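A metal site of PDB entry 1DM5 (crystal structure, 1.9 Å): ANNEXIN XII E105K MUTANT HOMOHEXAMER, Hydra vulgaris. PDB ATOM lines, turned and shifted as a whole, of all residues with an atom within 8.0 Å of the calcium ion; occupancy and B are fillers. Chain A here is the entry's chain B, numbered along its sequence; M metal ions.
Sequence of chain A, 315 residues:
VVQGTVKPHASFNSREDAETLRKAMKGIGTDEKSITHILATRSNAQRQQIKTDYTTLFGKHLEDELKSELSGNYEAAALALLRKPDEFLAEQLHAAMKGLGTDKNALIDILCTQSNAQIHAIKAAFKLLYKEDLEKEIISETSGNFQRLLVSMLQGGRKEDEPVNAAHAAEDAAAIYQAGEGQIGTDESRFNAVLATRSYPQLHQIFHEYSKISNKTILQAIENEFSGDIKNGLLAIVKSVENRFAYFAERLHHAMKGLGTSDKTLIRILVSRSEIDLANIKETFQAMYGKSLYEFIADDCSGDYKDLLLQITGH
O of Ile 184 touches the calcium ion, 3.3 Å away. Within 4 Å of the calcium ion: Gly 180, Gln 183, Ile 184, Gly 185 and Glu 225. The nearest printed residue that does not touch the calcium ion is Thr 186 (4.001 Å).
The side-chain amide oxygen (OE1) of Gln 183 is in hydrogen-bond range of the backbone NH (N) of Thr 186 (3.4 Å). The backbone carbonyl oxygen of Gly 185 lies close to the side-chain amide oxygen of Gln 183 (3.0 Å). NE2 of Gln 183 lies close to O of Gln 178, at 3.0 Å.
The calcium ion is bound by the side-chain carboxylate (OE2) of Glu 225 (2.5 Å), the backbone carbonyl oxygen (O) of Gly 180 (2.6 Å) and the backbone carbonyl oxygen (O) of Gln 183 (2.6 Å). The calcium ion has three donor atoms within binding distance. Slightly farther from the calcium ion lies O of Gly 185 (3.0 Å).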
ATOM      1  N   TYR A 177      28.081 -26.019  10.231  1.00  0.00           N
ATOM      2  CA  TYR A 177      28.603 -27.000  11.183  1.00  0.00           C
ATOM      3  C   TYR A 177      28.279 -26.638  12.631  1.00  0.00           C
ATOM      4  O   TYR A 177      27.883 -27.464  13.459  1.00  0.00           O
ATOM      5  CB  TYR A 177      30.114 -27.180  11.030  1.00  0.00           C
ATOM      6  CG  TYR A 177      30.648 -28.393  11.764  1.00  0.00           C
ATOM      7  CD1 TYR A 177      30.703 -29.628  11.147  1.00  0.00           C
ATOM      8  CD2 TYR A 177      31.085 -28.307  13.087  1.00  0.00           C
ATOM      9  CE1 TYR A 177      31.170 -30.754  11.810  1.00  0.00           C
ATOM     10  CE2 TYR A 177      31.562 -29.411  13.744  1.00  0.00           C
ATOM     11  CZ  TYR A 177      31.607 -30.644  13.118  1.00  0.00           C
ATOM     12  OH  TYR A 177      32.090 -31.738  13.790  1.00  0.00           O
ATOM     13  N   GLN A 178      28.509 -25.362  12.955  1.00  0.00           N
ATOM     14  CA  GLN A 178      28.312 -24.900  14.318  1.00  0.00           C
ATOM     15  C   GLN A 178      26.847 -24.890  14.723  1.00  0.00           C
ATOM     16  O   GLN A 178      26.519 -24.998  15.916  1.00  0.00           O
ATOM     17  CB  GLN A 178      28.918 -23.504  14.476  1.00  0.00           C
ATOM     18  CG  GLN A 178      30.431 -23.484  14.481  1.00  0.00           C
ATOM     19  CD  GLN A 178      31.022 -24.240  15.648  1.00  0.00           C
ATOM     20  OE1 GLN A 178      31.912 -25.073  15.465  1.00  0.00           O
ATOM     21  NE2 GLN A 178      30.543 -23.964  16.861  1.00  0.00           N
ATOM     22  N   ALA A 179      25.938 -24.756  13.759  1.00  0.00           N
ATOM     23  CA  ALA A 179      24.523 -24.639  14.119  1.00  0.00           C
ATOM     24  C   ALA A 179      23.869 -25.987  14.362  1.00  0.00           C
ATOM     25  O   ALA A 179      22.754 -26.079  14.866  1.00  0.00           O
ATOM     26  CB  ALA A 179      23.776 -23.812  13.087  1.00  0.00           C
ATOM     27  N   GLY A 180      24.538 -27.081  14.002  1.00  0.00           N
ATOM     28  CA  GLY A 180      24.000 -28.409  14.220  1.00  0.00           C
ATOM     29  C   GLY A 180      24.994 -29.287  14.963  1.00  0.00           C
ATOM     30  O   GLY A 180      25.077 -29.256  16.193  1.00  0.00           O
ATOM     31  N   GLU A 181      25.759 -30.056  14.210  1.00  0.00           N
ATOM     32  CA  GLU A 181      26.747 -30.994  14.700  1.00  0.00           C
ATOM     33  C   GLU A 181      27.611 -30.380  15.813  1.00  0.00           C
ATOM     34  O   GLU A 181      27.827 -31.013  16.837  1.00  0.00           O
ATOM     35  CB  GLU A 181      27.685 -31.362  13.546  1.00  0.00           C
ATOM     36  CG  GLU A 181      27.265 -32.527  12.686  1.00  0.00           C
ATOM     37  CD  GLU A 181      28.431 -32.945  11.790  1.00  0.00           C
ATOM     38  OE1 GLU A 181      28.467 -32.486  10.636  1.00  0.00           O
ATOM     39  OE2 GLU A 181      29.316 -33.665  12.304  1.00  0.00           O
ATOM     40  N   GLY A 182      28.114 -29.187  15.536  1.00  0.00           N
ATOM     41  CA  GLY A 182      29.033 -28.497  16.417  1.00  0.00           C
ATOM     42  C   GLY A 182      28.480 -28.206  17.794  1.00  0.00           C
ATOM     43  O   GLY A 182      29.265 -28.137  18.748  1.00  0.00           O
ATOM     44  N   GLN A 183      27.168 -28.009  17.926  1.00  0.00           N
ATOM     45  CA  GLN A 183      26.581 -27.608  19.203  1.00  0.00           C
ATOM     46  C   GLN A 183      25.574 -28.622  19.741  1.00  0.00           C
ATOM     47  O   GLN A 183      25.236 -29.588  19.057  1.00  0.00           O
ATOM     48  CB  GLN A 183      25.949 -26.225  19.078  1.00  0.00           C
ATOM     49  CG  GLN A 183      24.815 -26.075  18.084  1.00  0.00           C
ATOM     50  CD  GLN A 183      23.988 -24.831  18.305  1.00  0.00           C
ATOM     51  OE1 GLN A 183      23.112 -24.793  19.170  1.00  0.00           O
ATOM     52  NE2 GLN A 183      24.254 -23.776  17.530  1.00  0.00           N
ATOM     53  N   ILE A 184      25.160 -28.415  20.987  1.00  0.00           N
ATOM     54  CA  ILE A 184      24.233 -29.337  21.633  1.00  0.00           C
ATOM     55  C   ILE A 184      22.814 -29.056  21.148  1.00  0.00           C
ATOM     56  O   ILE A 184      22.115 -29.945  20.682  1.00  0.00           O
ATOM     57  CB  ILE A 184      24.210 -29.285  23.164  1.00  0.00           C
ATOM     58  CG1 ILE A 184      25.562 -29.370  23.878  1.00  0.00           C
ATOM     59  CG2 ILE A 184      23.282 -30.377  23.709  1.00  0.00           C
ATOM     60  CD1 ILE A 184      25.363 -29.381  25.387  1.00  0.00           C
ATOM     61  N   GLY A 185      22.405 -27.787  21.275  1.00  0.00           N
ATOM     62  CA  GLY A 185      21.116 -27.382  20.728  1.00  0.00           C
ATOM     63  C   GLY A 185      21.228 -27.198  19.226  1.00  0.00           C
ATOM     64  O   GLY A 185      22.209 -27.646  18.623  1.00  0.00           O
ATOM     65  N   THR A 186      20.260 -26.534  18.594  1.00  0.00           N
ATOM     66  CA  THR A 186      20.369 -26.308  17.156  1.00  0.00           C
ATOM     67  C   THR A 186      20.007 -24.869  16.799  1.00  0.00           C
ATOM     68  O   THR A 186      19.077 -24.296  17.371  1.00  0.00           O
ATOM     69  CB  THR A 186      19.439 -27.230  16.348  1.00  0.00           C
ATOM     70  OG1 THR A 186      19.630 -28.585  16.734  1.00  0.00           O
ATOM     71  CG2 THR A 186      19.770 -27.154  14.866  1.00  0.00           C
ATOM     72  N   ASP A 187      20.723 -24.312  15.825  1.00  0.00           N
ATOM     73  CA  ASP A 187      20.274 -23.065  15.225  1.00  0.00           C
ATOM     74  C   ASP A 187      19.685 -23.425  13.858  1.00  0.00           C
ATOM     75  O   ASP A 187      20.356 -23.323  12.830  1.00  0.00           O
ATOM     76  CB  ASP A 187      21.385 -22.038  15.045  1.00  0.00           C
ATOM     77  CG  ASP A 187      20.846 -20.752  14.444  1.00  0.00           C
ATOM     78  OD1 ASP A 187      21.661 -19.836  14.172  1.00  0.00           O
ATOM     79  OD2 ASP A 187      19.614 -20.648  14.258  1.00  0.00           O
ATOM     80  N   PHE A 191      20.570 -23.042   8.915  1.00  0.00           N
ATOM     81  CA  PHE A 191      20.246 -23.962   7.832  1.00  0.00           C
ATOM     82  C   PHE A 191      19.227 -23.304   6.891  1.00  0.00           C
ATOM     83  O   PHE A 191      19.394 -23.314   5.681  1.00  0.00           O
ATOM     84  CB  PHE A 191      19.618 -25.248   8.369  1.00  0.00           C
ATOM     85  CG  PHE A 191      20.576 -26.208   9.042  1.00  0.00           C
ATOM     86  CD1 PHE A 191      21.192 -27.208   8.332  1.00  0.00           C
ATOM     87  CD2 PHE A 191      20.839 -26.096  10.397  1.00  0.00           C
ATOM     88  CE1 PHE A 191      22.054 -28.087   8.965  1.00  0.00           C
ATOM     89  CE2 PHE A 191      21.698 -26.963  11.036  1.00  0.00           C
ATOM     90  CZ  PHE A 191      22.311 -27.969  10.318  1.00  0.00           C
ATOM     91  N   ALA A 221      24.224 -34.839   7.962  1.00  0.00           N
ATOM     92  CA  ALA A 221      24.161 -33.799   8.986  1.00  0.00           C
ATOM     93  C   ALA A 221      22.726 -33.356   9.260  1.00  0.00           C
ATOM     94  O   ALA A 221      22.276 -33.215  10.399  1.00  0.00           O
ATOM     95  CB  ALA A 221      25.013 -32.616   8.528  1.00  0.00           C
ATOM     96  N   ASN A 224      20.669 -36.159  10.719  1.00  0.00           N
ATOM     97  CA  ASN A 224      21.073 -36.213  12.115  1.00  0.00           C
ATOM     98  C   ASN A 224      20.420 -35.117  12.943  1.00  0.00           C
ATOM     99  O   ASN A 224      19.944 -35.393  14.045  1.00  0.00           O
ATOM    100  CB  ASN A 224      22.600 -36.111  12.213  1.00  0.00           C
ATOM    101  CG  ASN A 224      23.183 -36.772  13.446  1.00  0.00           C
ATOM    102  OD1 ASN A 224      23.608 -37.932  13.405  1.00  0.00           O
ATOM    103  ND2 ASN A 224      23.231 -36.044  14.548  1.00  0.00           N
ATOM    104  N   GLU A 225      20.379 -33.871  12.451  1.00  0.00           N
ATOM    105  CA  GLU A 225      19.909 -32.762  13.255  1.00  0.00           C
ATOM    106  C   GLU A 225      18.395 -32.559  13.290  1.00  0.00           C
ATOM    107  O   GLU A 225      17.868 -31.878  14.182  1.00  0.00           O
ATOM    108  CB  GLU A 225      20.547 -31.460  12.742  1.00  0.00           C
ATOM    109  CG  GLU A 225      20.486 -30.320  13.762  1.00  0.00           C
ATOM    110  CD  GLU A 225      21.489 -30.535  14.881  1.00  0.00           C
ATOM    111  OE1 GLU A 225      22.410 -31.361  14.719  1.00  0.00           O
ATOM    112  OE2 GLU A 225      21.348 -29.879  15.921  1.00  0.00           O
HETATM  113 CA    CA M   1      23.168 -30.245  17.591  1.00  0.00          CA
